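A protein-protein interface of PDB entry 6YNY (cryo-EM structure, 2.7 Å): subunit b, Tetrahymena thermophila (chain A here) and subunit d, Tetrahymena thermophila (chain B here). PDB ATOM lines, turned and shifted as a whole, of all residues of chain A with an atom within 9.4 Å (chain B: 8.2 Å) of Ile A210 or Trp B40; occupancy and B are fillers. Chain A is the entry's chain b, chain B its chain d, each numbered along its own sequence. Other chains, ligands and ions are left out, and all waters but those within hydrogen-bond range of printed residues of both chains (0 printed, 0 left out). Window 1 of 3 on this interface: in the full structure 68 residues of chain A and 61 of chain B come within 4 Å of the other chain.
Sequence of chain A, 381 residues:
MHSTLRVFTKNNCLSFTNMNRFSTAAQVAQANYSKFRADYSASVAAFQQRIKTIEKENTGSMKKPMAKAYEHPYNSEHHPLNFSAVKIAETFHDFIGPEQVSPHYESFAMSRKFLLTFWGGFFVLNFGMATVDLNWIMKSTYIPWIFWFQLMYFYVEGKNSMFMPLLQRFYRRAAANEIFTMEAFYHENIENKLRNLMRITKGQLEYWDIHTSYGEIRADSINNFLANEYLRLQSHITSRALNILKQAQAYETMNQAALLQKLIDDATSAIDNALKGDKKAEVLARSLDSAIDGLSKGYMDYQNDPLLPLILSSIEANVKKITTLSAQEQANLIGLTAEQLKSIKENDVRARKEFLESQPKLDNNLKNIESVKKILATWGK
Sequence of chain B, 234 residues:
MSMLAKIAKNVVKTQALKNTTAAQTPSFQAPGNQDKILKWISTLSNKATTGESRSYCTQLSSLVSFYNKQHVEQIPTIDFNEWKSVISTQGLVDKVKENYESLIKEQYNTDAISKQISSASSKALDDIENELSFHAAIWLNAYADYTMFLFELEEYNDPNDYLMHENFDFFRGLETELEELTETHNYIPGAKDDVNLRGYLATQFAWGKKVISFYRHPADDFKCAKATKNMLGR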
ATOM      1  N   GLY A 203      32.998 -27.542  27.214  1.00  0.00           N
ATOM      2  CA  GLY A 203      32.735 -27.975  25.854  1.00  0.00           C
ATOM      3  C   GLY A 203      31.424 -28.718  25.711  1.00  0.00           C
ATOM      4  O   GLY A 203      30.754 -28.605  24.682  1.00  0.00           O
ATOM      5  N   GLN A 204      31.044 -29.489  26.726  1.00  0.00           N
ATOM      6  CA  GLN A 204      29.777 -30.199  26.699  1.00  0.00           C
ATOM      7  C   GLN A 204      28.594 -29.288  26.976  1.00  0.00           C
ATOM      8  O   GLN A 204      27.475 -29.601  26.560  1.00  0.00           O
ATOM      9  CB  GLN A 204      29.795 -31.338  27.715  1.00  0.00           C
ATOM     10  CG  GLN A 204      30.670 -32.498  27.317  1.00  0.00           C
ATOM     11  CD  GLN A 204      30.127 -33.247  26.127  1.00  0.00           C
ATOM     12  OE1 GLN A 204      28.981 -33.692  26.128  1.00  0.00           O
ATOM     13  NE2 GLN A 204      30.944 -33.381  25.095  1.00  0.00           N
ATOM     14  N   LEU A 205      28.815 -28.175  27.667  1.00  0.00           N
ATOM     15  CA  LEU A 205      27.755 -27.219  27.944  1.00  0.00           C
ATOM     16  C   LEU A 205      27.441 -26.316  26.760  1.00  0.00           C
ATOM     17  O   LEU A 205      26.467 -25.560  26.821  1.00  0.00           O
ATOM     18  CB  LEU A 205      28.139 -26.368  29.151  1.00  0.00           C
ATOM     19  CG  LEU A 205      28.301 -27.135  30.460  1.00  0.00           C
ATOM     20  CD1 LEU A 205      28.949 -26.273  31.506  1.00  0.00           C
ATOM     21  CD2 LEU A 205      26.970 -27.626  30.959  1.00  0.00           C
ATOM     22  N   GLU A 206      28.238 -26.372  25.693  1.00  0.00           N
ATOM     23  CA  GLU A 206      27.961 -25.569  24.510  1.00  0.00           C
ATOM     24  C   GLU A 206      26.701 -26.017  23.786  1.00  0.00           C
ATOM     25  O   GLU A 206      26.141 -25.241  23.007  1.00  0.00           O
ATOM     26  CB  GLU A 206      29.147 -25.631  23.550  1.00  0.00           C
ATOM     27  CG  GLU A 206      30.431 -25.065  24.111  1.00  0.00           C
ATOM     28  CD  GLU A 206      31.600 -25.224  23.164  1.00  0.00           C
ATOM     29  OE1 GLU A 206      31.388 -25.707  22.032  1.00  0.00           O
ATOM     30  OE2 GLU A 206      32.733 -24.868  23.551  1.00  0.00           O
ATOM     31  N   TYR A 207      26.247 -27.246  24.024  1.00  0.00           N
ATOM     32  CA  TYR A 207      25.069 -27.755  23.334  1.00  0.00           C
ATOM     33  C   TYR A 207      23.781 -27.186  23.911  1.00  0.00           C
ATOM     34  O   TYR A 207      22.834 -26.913  23.166  1.00  0.00           O
ATOM     35  CB  TYR A 207      25.052 -29.280  23.402  1.00  0.00           C
ATOM     36  CG  TYR A 207      26.222 -29.940  22.716  1.00  0.00           C
ATOM     37  CD1 TYR A 207      27.447 -30.055  23.350  1.00  0.00           C
ATOM     38  CD2 TYR A 207      26.099 -30.456  21.437  1.00  0.00           C
ATOM     39  CE1 TYR A 207      28.516 -30.657  22.729  1.00  0.00           C
ATOM     40  CE2 TYR A 207      27.163 -31.060  20.808  1.00  0.00           C
ATOM     41  CZ  TYR A 207      28.367 -31.161  21.460  1.00  0.00           C
ATOM     42  OH  TYR A 207      29.433 -31.761  20.836  1.00  0.00           O
ATOM     43  N   TRP A 208      23.721 -27.003  25.229  1.00  0.00           N
ATOM     44  CA  TRP A 208      22.514 -26.458  25.836  1.00  0.00           C
ATOM     45  C   TRP A 208      22.317 -24.994  25.477  1.00  0.00           C
ATOM     46  O   TRP A 208      21.177 -24.522  25.408  1.00  0.00           O
ATOM     47  CB  TRP A 208      22.572 -26.629  27.351  1.00  0.00           C
ATOM     48  CG  TRP A 208      21.377 -26.098  28.065  1.00  0.00           C
ATOM     49  CD1 TRP A 208      21.333 -25.022  28.895  1.00  0.00           C
ATOM     50  CD2 TRP A 208      20.046 -26.615  28.009  1.00  0.00           C
ATOM     51  NE1 TRP A 208      20.059 -24.838  29.365  1.00  0.00           N
ATOM     52  CE2 TRP A 208      19.249 -25.804  28.834  1.00  0.00           C
ATOM     53  CE3 TRP A 208      19.449 -27.687  27.342  1.00  0.00           C
ATOM     54  CZ2 TRP A 208      17.890 -26.028  29.007  1.00  0.00           C
ATOM     55  CZ3 TRP A 208      18.105 -27.906  27.517  1.00  0.00           C
ATOM     56  CH2 TRP A 208      17.339 -27.083  28.343  1.00  0.00           C
ATOM     57  N   ASP A 209      23.405 -24.263  25.244  1.00  0.00           N
ATOM     58  CA  ASP A 209      23.284 -22.869  24.837  1.00  0.00           C
ATOM     59  C   ASP A 209      22.733 -22.748  23.425  1.00  0.00           C
ATOM     60  O   ASP A 209      22.119 -21.731  23.084  1.00  0.00           O
ATOM     61  CB  ASP A 209      24.642 -22.181  24.935  1.00  0.00           C
ATOM     62  CG  ASP A 209      25.209 -22.207  26.340  1.00  0.00           C
ATOM     63  OD1 ASP A 209      24.501 -22.664  27.260  1.00  0.00           O
ATOM     64  OD2 ASP A 209      26.366 -21.775  26.523  1.00  0.00           O
ATOM     65  N   ILE A 210      22.938 -23.769  22.596  1.00  0.00           N
ATOM     66  CA  ILE A 210      22.450 -23.733  21.223  1.00  0.00           C
ATOM     67  C   ILE A 210      20.958 -24.026  21.170  1.00  0.00           C
ATOM     68  O   ILE A 210      20.220 -23.406  20.399  1.00  0.00           O
ATOM     69  CB  ILE A 210      23.252 -24.727  20.366  1.00  0.00           C
ATOM     70  CG1 ILE A 210      24.713 -24.288  20.277  1.00  0.00           C
ATOM     71  CG2 ILE A 210      22.643 -24.849  18.989  1.00  0.00           C
ATOM     72  CD1 ILE A 210      25.625 -25.325  19.680  1.00  0.00           C
ATOM     73  N   HIS A 211      20.493 -24.972  21.984  1.00  0.00           N
ATOM     74  CA  HIS A 211      19.086 -25.348  21.960  1.00  0.00           C
ATOM     75  C   HIS A 211      18.196 -24.253  22.527  1.00  0.00           C
ATOM     76  O   HIS A 211      17.025 -24.148  22.144  1.00  0.00           O
ATOM     77  CB  HIS A 211      18.889 -26.644  22.738  1.00  0.00           C
ATOM     78  CG  HIS A 211      17.456 -27.028  22.917  1.00  0.00           C
ATOM     79  ND1 HIS A 211      16.675 -27.491  21.882  1.00  0.00           N
ATOM     80  CD2 HIS A 211      16.662 -27.018  24.011  1.00  0.00           C
ATOM     81  CE1 HIS A 211      15.461 -27.750  22.331  1.00  0.00           C
ATOM     82  NE2 HIS A 211      15.427 -27.472  23.621  1.00  0.00           N
ATOM     83  N   THR A 212      18.722 -23.434  23.437  1.00  0.00           N
ATOM     84  CA  THR A 212      17.920 -22.370  24.029  1.00  0.00           C
ATOM     85  C   THR A 212      17.514 -21.325  23.000  1.00  0.00           C
ATOM     86  O   THR A 212      16.478 -20.670  23.162  1.00  0.00           O
ATOM     87  CB  THR A 212      18.691 -21.705  25.163  1.00  0.00           C
ATOM     88  OG1 THR A 212      20.008 -21.365  24.714  1.00  0.00           O
ATOM     89  CG2 THR A 212      18.784 -22.630  26.351  1.00  0.00           C
ATOM     90  N   SER A 213      18.304 -21.155  21.945  1.00  0.00           N
ATOM     91  CA  SER A 213      18.009 -20.174  20.913  1.00  0.00           C
ATOM     92  C   SER A 213      17.144 -20.726  19.790  1.00  0.00           C
ATOM     93  O   SER A 213      16.721 -19.957  18.923  1.00  0.00           O
ATOM     94  CB  SER A 213      19.313 -19.633  20.330  1.00  0.00           C
ATOM     95  OG  SER A 213      20.112 -19.050  21.343  1.00  0.00           O
ATOM     96  N   TYR A 214      16.865 -22.030  19.786  1.00  0.00           N
ATOM     97  CA  TYR A 214      16.050 -22.606  18.724  1.00  0.00           C
ATOM     98  C   TYR A 214      14.656 -21.996  18.708  1.00  0.00           C
ATOM     99  O   TYR A 214      14.097 -21.735  17.636  1.00  0.00           O
ATOM    100  CB  TYR A 214      15.970 -24.121  18.897  1.00  0.00           C
ATOM    101  CG  TYR A 214      15.069 -24.816  17.904  1.00  0.00           C
ATOM    102  CD1 TYR A 214      15.477 -25.030  16.596  1.00  0.00           C
ATOM    103  CD2 TYR A 214      13.814 -25.271  18.279  1.00  0.00           C
ATOM    104  CE1 TYR A 214      14.657 -25.668  15.690  1.00  0.00           C
ATOM    105  CE2 TYR A 214      12.989 -25.910  17.381  1.00  0.00           C
ATOM    106  CZ  TYR A 214      13.416 -26.107  16.088  1.00  0.00           C
ATOM    107  OH  TYR A 214      12.593 -26.746  15.190  1.00  0.00           O
ATOM    108  N   GLY A 215      14.077 -21.763  19.884  1.00  0.00           N
ATOM    109  CA  GLY A 215      12.773 -21.122  19.936  1.00  0.00           C
ATOM    110  C   GLY A 215      12.799 -19.708  19.393  1.00  0.00           C
ATOM    111  O   GLY A 215      11.842 -19.259  18.757  1.00  0.00           O
ATOM    112  N   GLU A 216      13.894 -18.987  19.634  1.00  0.00           N
ATOM    113  CA  GLU A 216      14.012 -17.632  19.105  1.00  0.00           C
ATOM    114  C   GLU A 216      14.243 -17.658  17.601  1.00  0.00           C
ATOM    115  O   GLU A 216      13.743 -16.792  16.874  1.00  0.00           O
ATOM    116  CB  GLU A 216      15.147 -16.896  19.816  1.00  0.00           C
ATOM    117  CG  GLU A 216      15.268 -15.421  19.463  1.00  0.00           C
ATOM    118  CD  GLU A 216      16.008 -15.177  18.159  1.00  0.00           C
ATOM    119  OE1 GLU A 216      16.662 -16.115  17.655  1.00  0.00           O
ATOM    120  OE2 GLU A 216      15.931 -14.046  17.636  1.00  0.00           O
ATOM    121  N   ILE A 217      14.995 -18.644  17.118  1.00  0.00           N
ATOM    122  CA  ILE A 217      15.235 -18.765  15.685  1.00  0.00           C
ATOM    123  C   ILE A 217      13.966 -19.203  14.970  1.00  0.00           C
ATOM    124  O   ILE A 217      13.647 -18.710  13.881  1.00  0.00           O
ATOM    125  CB  ILE A 217      16.396 -19.743  15.425  1.00  0.00           C
ATOM    126  CG1 ILE A 217      17.704 -19.194  16.002  1.00  0.00           C
ATOM    127  CG2 ILE A 217      16.534 -20.020  13.943  1.00  0.00           C
ATOM    128  CD1 ILE A 217      18.173 -17.911  15.376  1.00  0.00           C
ATOM    129  N   ARG A 218      13.223 -20.135  15.566  1.00  0.00           N
ATOM    130  CA  ARG A 218      12.001 -20.620  14.938  1.00  0.00           C
ATOM    131  C   ARG A 218      10.954 -19.522  14.820  1.00  0.00           C
ATOM    132  O   ARG A 218      10.196 -19.491  13.845  1.00  0.00           O
ATOM    133  CB  ARG A 218      11.438 -21.795  15.733  1.00  0.00           C
ATOM    134  CG  ARG A 218      10.251 -22.461  15.077  1.00  0.00           C
ATOM    135  CD  ARG A 218       9.750 -23.638  15.889  1.00  0.00           C
ATOM    136  NE  ARG A 218       9.245 -23.229  17.194  1.00  0.00           N
ATOM    137  CZ  ARG A 218       8.647 -24.048  18.051  1.00  0.00           C
ATOM    138  NH1 ARG A 218       8.476 -25.326  17.742  1.00  0.00           N
ATOM    139  NH2 ARG A 218       8.216 -23.591  19.217  1.00  0.00           N
ATOM    140  N   SER A 221      12.131 -17.023  12.094  1.00  0.00           N
ATOM    141  CA  SER A 221      12.126 -17.648  10.777  1.00  0.00           C
ATOM    142  C   SER A 221      10.719 -17.698  10.197  1.00  0.00           C
ATOM    143  O   SER A 221      10.534 -17.529   8.986  1.00  0.00           O
ATOM    144  CB  SER A 221      12.719 -19.052  10.861  1.00  0.00           C
ATOM    145  OG  SER A 221      14.084 -19.005  11.237  1.00  0.00           O
ATOM    146  N   GLN B  34      18.641 -11.138   9.669  1.00  0.00           N
ATOM    147  CA  GLN B  34      19.024 -12.536   9.541  1.00  0.00           C
ATOM    148  C   GLN B  34      20.463 -12.797   9.959  1.00  0.00           C
ATOM    149  O   GLN B  34      20.925 -13.939   9.849  1.00  0.00           O
ATOM    150  CB  GLN B  34      18.825 -13.009   8.095  1.00  0.00           C
ATOM    151  CG  GLN B  34      17.391 -12.921   7.610  1.00  0.00           C
ATOM    152  CD  GLN B  34      17.228 -13.405   6.184  1.00  0.00           C
ATOM    153  OE1 GLN B  34      18.191 -13.824   5.544  1.00  0.00           O
ATOM    154  NE2 GLN B  34      16.001 -13.347   5.678  1.00  0.00           N
ATOM    155  N   ASP B  35      21.183 -11.781  10.438  1.00  0.00           N
ATOM    156  CA  ASP B  35      22.577 -11.975  10.818  1.00  0.00           C
ATOM    157  C   ASP B  35      22.697 -12.931  11.999  1.00  0.00           C
ATOM    158  O   ASP B  35      23.523 -13.852  11.987  1.00  0.00           O
ATOM    159  CB  ASP B  35      23.214 -10.626  11.147  1.00  0.00           C
ATOM    160  CG  ASP B  35      23.106  -9.638  10.004  1.00  0.00           C
ATOM    161  OD1 ASP B  35      22.558 -10.011   8.946  1.00  0.00           O
ATOM    162  OD2 ASP B  35      23.566  -8.488  10.163  1.00  0.00           O
ATOM    163  N   LYS B  36      21.875 -12.728  13.029  1.00  0.00           N
ATOM    164  CA  LYS B  36      21.941 -13.588  14.205  1.00  0.00           C
ATOM    165  C   LYS B  36      21.585 -15.025  13.853  1.00  0.00           C
ATOM    166  O   LYS B  36      22.167 -15.970  14.396  1.00  0.00           O
ATOM    167  CB  LYS B  36      21.008 -13.061  15.293  1.00  0.00           C
ATOM    168  CG  LYS B  36      21.266 -11.612  15.678  1.00  0.00           C
ATOM    169  CD  LYS B  36      20.352 -11.146  16.808  1.00  0.00           C
ATOM    170  CE  LYS B  36      18.877 -11.214  16.426  1.00  0.00           C
ATOM    171  NZ  LYS B  36      18.574 -10.480  15.167  1.00  0.00           N
ATOM    172  N   ILE B  37      20.627 -15.208  12.943  1.00  0.00           N
ATOM    173  CA  ILE B  37      20.202 -16.548  12.564  1.00  0.00           C
ATOM    174  C   ILE B  37      21.317 -17.311  11.867  1.00  0.00           C
ATOM    175  O   ILE B  37      21.303 -18.548  11.857  1.00  0.00           O
ATOM    176  CB  ILE B  37      18.950 -16.479  11.670  1.00  0.00           C
ATOM    177  CG1 ILE B  37      17.818 -15.756  12.405  1.00  0.00           C
ATOM    178  CG2 ILE B  37      18.521 -17.877  11.263  1.00  0.00           C
ATOM    179  CD1 ILE B  37      16.597 -15.486  11.554  1.00  0.00           C
ATOM    180  N   LEU B  38      22.287 -16.610  11.281  1.00  0.00           N
ATOM    181  CA  LEU B  38      23.380 -17.289  10.596  1.00  0.00           C
ATOM    182  C   LEU B  38      24.431 -17.798  11.573  1.00  0.00           C
ATOM    183  O   LEU B  38      25.064 -18.827  11.312  1.00  0.00           O
ATOM    184  CB  LEU B  38      24.026 -16.351   9.579  1.00  0.00           C
ATOM    185  CG  LEU B  38      23.136 -15.928   8.409  1.00  0.00           C
ATOM    186  CD1 LEU B  38      23.879 -14.958   7.510  1.00  0.00           C
ATOM    187  CD2 LEU B  38      22.658 -17.135   7.620  1.00  0.00           C
ATOM    188  N   LYS B  39      24.632 -17.100  12.691  1.00  0.00           N
ATOM    189  CA  LYS B  39      25.612 -17.554  13.669  1.00  0.00           C
ATOM    190  C   LYS B  39      25.149 -18.839  14.340  1.00  0.00           C
ATOM    191  O   LYS B  39      25.949 -19.753  14.567  1.00  0.00           O
ATOM    192  CB  LYS B  39      25.859 -16.466  14.713  1.00  0.00           C
ATOM    193  CG  LYS B  39      26.014 -15.067  14.140  1.00  0.00           C
ATOM    194  CD  LYS B  39      27.091 -15.008  13.071  1.00  0.00           C
ATOM    195  CE  LYS B  39      27.209 -13.610  12.488  1.00  0.00           C
ATOM    196  NZ  LYS B  39      28.250 -13.531  11.427  1.00  0.00           N
ATOM    197  N   TRP B  40      23.857 -18.927  14.656  1.00  0.00           N
ATOM    198  CA  TRP B  40      23.329 -20.119  15.306  1.00  0.00           C
ATOM    199  C   TRP B  40      23.515 -21.348  14.429  1.00  0.00           C
ATOM    200  O   TRP B  40      23.926 -22.410  14.910  1.00  0.00           O
ATOM    201  CB  TRP B  40      21.853 -19.911  15.634  1.00  0.00           C
ATOM    202  CG  TRP B  40      21.217 -21.044  16.361  1.00  0.00           C
ATOM    203  CD1 TRP B  40      21.183 -21.232  17.708  1.00  0.00           C
ATOM    204  CD2 TRP B  40      20.510 -22.146  15.784  1.00  0.00           C
ATOM    205  NE1 TRP B  40      20.500 -22.382  18.009  1.00  0.00           N
ATOM    206  CE2 TRP B  40      20.078 -22.964  16.843  1.00  0.00           C
ATOM    207  CE3 TRP B  40      20.204 -22.521  14.475  1.00  0.00           C
ATOM    208  CZ2 TRP B  40      19.356 -24.133  16.634  1.00  0.00           C
ATOM    209  CZ3 TRP B  40      19.487 -23.681  14.270  1.00  0.00           C
ATOM    210  CH2 TRP B  40      19.071 -24.474  15.342  1.00  0.00           C
ATOM    211  N   ILE B  41      23.217 -21.223  13.135  1.00  0.00           N
ATOM    212  CA  ILE B  41      23.346 -22.364  12.237  1.00  0.00           C
ATOM    213  C   ILE B  41      24.812 -22.707  12.013  1.00  0.00           C
ATOM    214  O   ILE B  41      25.165 -23.883  11.862  1.00  0.00           O
ATOM    215  CB  ILE B  41      22.621 -22.075  10.909  1.00  0.00           C
ATOM    216  CG1 ILE B  41      22.693 -23.281   9.973  1.00  0.00           C
ATOM    217  CG2 ILE B  41      23.219 -20.862  10.228  1.00  0.00           C
ATOM    218  CD1 ILE B  41      22.085 -24.532  10.545  1.00  0.00           C
ATOM    219  N   SER B  42      25.685 -21.700  11.981  1.00  0.00           N
ATOM    220  CA  SER B  42      27.104 -21.962  11.762  1.00  0.00           C
ATOM    221  C   SER B  42      27.684 -22.788  12.901  1.00  0.00           C
ATOM    222  O   SER B  42      28.357 -23.800  12.673  1.00  0.00           O
ATOM    223  CB  SER B  42      27.862 -20.644  11.616  1.00  0.00           C
ATOM    224  OG  SER B  42      27.829 -19.907  12.823  1.00  0.00           O
ATOM    225  N   THR B  43      27.432 -22.368  14.143  1.00  0.00           N
ATOM    226  CA  THR B  43      27.912 -23.129  15.290  1.00  0.00           C
ATOM    227  C   THR B  43      27.290 -24.515  15.321  1.00  0.00           C
ATOM    228  O   THR B  43      27.969 -25.505  15.615  1.00  0.00           O
ATOM    229  CB  THR B  43      27.596 -22.381  16.582  1.00  0.00           C
ATOM    230  OG1 THR B  43      26.178 -22.232  16.713  1.00  0.00           O
ATOM    231  CG2 THR B  43      28.246 -21.010  16.578  1.00  0.00           C
ATOM    232  N   LEU B  44      25.995 -24.606  15.019  1.00  0.00           N
ATOM    233  CA  LEU B  44      25.330 -25.902  15.004  1.00  0.00           C
ATOM    234  C   LEU B  44      25.974 -26.832  13.986  1.00  0.00           C
ATOM    235  O   LEU B  44      26.134 -28.030  14.241  1.00  0.00           O
ATOM    236  CB  LEU B  44      23.844 -25.706  14.705  1.00  0.00           C
ATOM    237  CG  LEU B  44      22.910 -26.918  14.720  1.00  0.00           C
ATOM    238  CD1 LEU B  44      23.060 -27.746  13.460  1.00  0.00           C
ATOM    239  CD2 LEU B  44      23.156 -27.772  15.943  1.00  0.00           C
ATOM    240  N   SER B  45      26.354 -26.297  12.825  1.00  0.00           N
ATOM    241  CA  SER B  45      26.956 -27.127  11.788  1.00  0.00           C
ATOM    242  C   SER B  45      28.400 -27.477  12.119  1.00  0.00           C
ATOM    243  O   SER B  45      28.846 -28.599  11.850  1.00  0.00           O
ATOM    244  CB  SER B  45      26.879 -26.416  10.438  1.00  0.00           C
ATOM    245  OG  SER B  45      25.534 -26.201  10.053  1.00  0.00           O
ATOM    246  N   ASN B  46      29.148 -26.534  12.695  1.00  0.00           N
ATOM    247  CA  ASN B  46      30.541 -26.808  13.029  1.00  0.00           C
ATOM    248  C   ASN B  46      30.662 -27.945  14.033  1.00  0.00           C
ATOM    249  O   ASN B  46      31.638 -28.702  14.001  1.00  0.00           O
ATOM    250  CB  ASN B  46      31.206 -25.548  13.576  1.00  0.00           C
ATOM    251  CG  ASN B  46      31.255 -24.429  12.556  1.00  0.00           C
ATOM    252  OD1 ASN B  46      31.284 -24.673  11.351  1.00  0.00           O
ATOM    253  ND2 ASN B  46      31.267 -23.193  13.036  1.00  0.00           N
ATOM    254  N   LYS B  47      29.684 -28.081  14.930  1.00  0.00           N
ATOM    255  CA  LYS B  47      29.721 -29.155  15.913  1.00  0.00           C
ATOM    256  C   LYS B  47      29.455 -30.512  15.278  1.00  0.00           C
ATOM    257  O   LYS B  47      29.780 -31.540  15.881  1.00  0.00           O
ATOM    258  CB  LYS B  47      28.703 -28.891  17.020  1.00  0.00           C
ATOM    259  CG  LYS B  47      28.978 -27.632  17.829  1.00  0.00           C
ATOM    260  CD  LYS B  47      30.168 -27.787  18.752  1.00  0.00           C
ATOM    261  CE  LYS B  47      29.836 -28.648  19.950  1.00  0.00           C
ATOM    262  NZ  LYS B  47      31.001 -28.807  20.860  1.00  0.00           N
ATOM    263  N   CYS B  57      22.061 -31.283   9.101  1.00  0.00           N
ATOM    264  CA  CYS B  57      22.393 -29.864   9.163  1.00  0.00           C
ATOM    265  C   CYS B  57      22.100 -29.176   7.838  1.00  0.00           C
ATOM    266  O   CYS B  57      21.629 -28.033   7.816  1.00  0.00           O
ATOM    267  CB  CYS B  57      23.861 -29.685   9.544  1.00  0.00           C
ATOM    268  SG  CYS B  57      24.219 -30.009  11.281  1.00  0.00           S
ATOM    269  N   LEU B  60      18.384 -28.751   7.623  1.00  0.00           N
ATOM    270  CA  LEU B  60      17.977 -27.648   8.482  1.00  0.00           C
ATOM    271  C   LEU B  60      18.302 -26.306   7.841  1.00  0.00           C
ATOM    272  O   LEU B  60      17.507 -25.364   7.913  1.00  0.00           O
ATOM    273  CB  LEU B  60      18.657 -27.782   9.845  1.00  0.00           C
ATOM    274  CG  LEU B  60      18.214 -26.871  10.993  1.00  0.00           C
ATOM    275  CD1 LEU B  60      18.649 -25.437  10.766  1.00  0.00           C
ATOM    276  CD2 LEU B  60      16.710 -26.948  11.187  1.00  0.00           C
ATOM    277  N   SER B  61      19.469 -26.202   7.203  1.00  0.00           N
ATOM    278  CA  SER B  61      19.854 -24.942   6.578  1.00  0.00           C
ATOM    279  C   SER B  61      18.901 -24.573   5.450  1.00  0.00           C
ATOM    280  O   SER B  61      18.558 -23.398   5.274  1.00  0.00           O
ATOM    281  CB  SER B  61      21.287 -25.030   6.060  1.00  0.00           C
ATOM    282  OG  SER B  61      21.703 -23.795   5.510  1.00  0.00           O
ATOM    283  N   VAL B  64      15.714 -23.090   6.819  1.00  0.00           N
ATOM    284  CA  VAL B  64      15.925 -21.728   7.297  1.00  0.00           C
ATOM    285  C   VAL B  64      15.973 -20.761   6.123  1.00  0.00           C
ATOM    286  O   VAL B  64      15.303 -19.722   6.124  1.00  0.00           O
ATOM    287  CB  VAL B  64      17.208 -21.651   8.142  1.00  0.00           C
ATOM    288  CG1 VAL B  64      17.509 -20.213   8.519  1.00  0.00           C
ATOM    289  CG2 VAL B  64      17.070 -22.508   9.387  1.00  0.00           C
ATOM    290  N   LEU B 132      18.852 -33.068  26.680  1.00  0.00           N
ATOM    291  CA  LEU B 132      19.928 -32.102  26.848  1.00  0.00           C
ATOM    292  C   LEU B 132      19.893 -31.440  28.214  1.00  0.00           C
ATOM    293  O   LEU B 132      20.929 -30.963  28.687  1.00  0.00           O
ATOM    294  CB  LEU B 132      19.855 -31.039  25.756  1.00  0.00           C
ATOM    295  CG  LEU B 132      20.168 -31.509  24.340  1.00  0.00           C
ATOM    296  CD1 LEU B 132      19.936 -30.384  23.368  1.00  0.00           C
ATOM    297  CD2 LEU B 132      21.594 -32.004  24.231  1.00  0.00           C
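O of Ile A210 sits at hydrogen-bond distance from NE1 of Trp B40 (2.6 Å). The side-chain amino group (NZ) of Lys B47 is in salt-bridge range of the side-chain carboxylate (OE1) of Glu A206, 3.3 Å away. OH of Tyr A207 sits close to NZ of Lys B47, 3.3 Å away.
O of Ile A217 is in hydrogen-bond range of OG of Ser A221 (2.7 Å). The backbone carbonyl oxygen (O) of Trp B40 lies within hydrogen-bond range of the side-chain hydroxyl (OG1) of Thr B43, 2.9 Å away. OG1 of Thr A212 sits close to O of Trp A208 (3.4 Å).
Gly A203 touches Lys B47 (O to NZ, 3.8 Å). CB of Leu B132 touches CE3 of Trp A208, 3.7 Å away. CD1 of Leu B132 touches CB of His A211, 3.9 Å away. CD1 of Trp B40 touches CB of Ser A213 (3.6 Å). Trp B40 touches Tyr A214 (CH2 to CD1, 3.8 Å). CD1 of Ile A217 touches CG1 of Ile B37 (3.7 Å). CG1 of Ile A217 touches CG of Trp B40 (3.99 Å).
Of the printed residues of chain B, Ile A210 touches Trp B40. Of the printed residues of chain A, Trp B40 touches Ile A210, Ser A213, Tyr A214 and Ile A217. No residue of chain A comes within 4 Å of Ile B41. No residue of chain A comes within 4 Å of Ser B42. No residue of chain A comes within 4 Å of Thr B43. Printed residues of chain B within 4 Å of Glu A206: Lys B47. Printed residues of chain A within 4 Å of Leu B132: Trp A208 (3.7 Å) and His A211 (3.9 Å). Of the printed residues of chain A, Ile B37 touches Ile A217. Printed residues of chain B within 4 Å of His A211: Leu B132. The nearest residue of chain B that does not touch Ile A210 is Leu B44 (4.3 Å).
Printed residues of chain B that touch a printed residue of chain A: Ile B37, Trp B40, Lys B47 and Leu B132. Hydrophobic or aromatic side chains of chain B within 4 Å of the printed part of chain A: Ile B37, Trp B40 and Leu B132. Hydrophobic or aromatic side chains of chain A within 4 Å of the printed part of chain B: Tyr A207, Trp A208, Ile A210, His A211, Tyr A214 and Ile A217. Among the printed residues, 10 pairs touch across the chains. Among the printed residues, Asp or Glu carboxylates within 4 Å of a Lys or Arg side-chain nitrogen of the other chain: Glu A206 with Lys B47 (3.3 Å).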
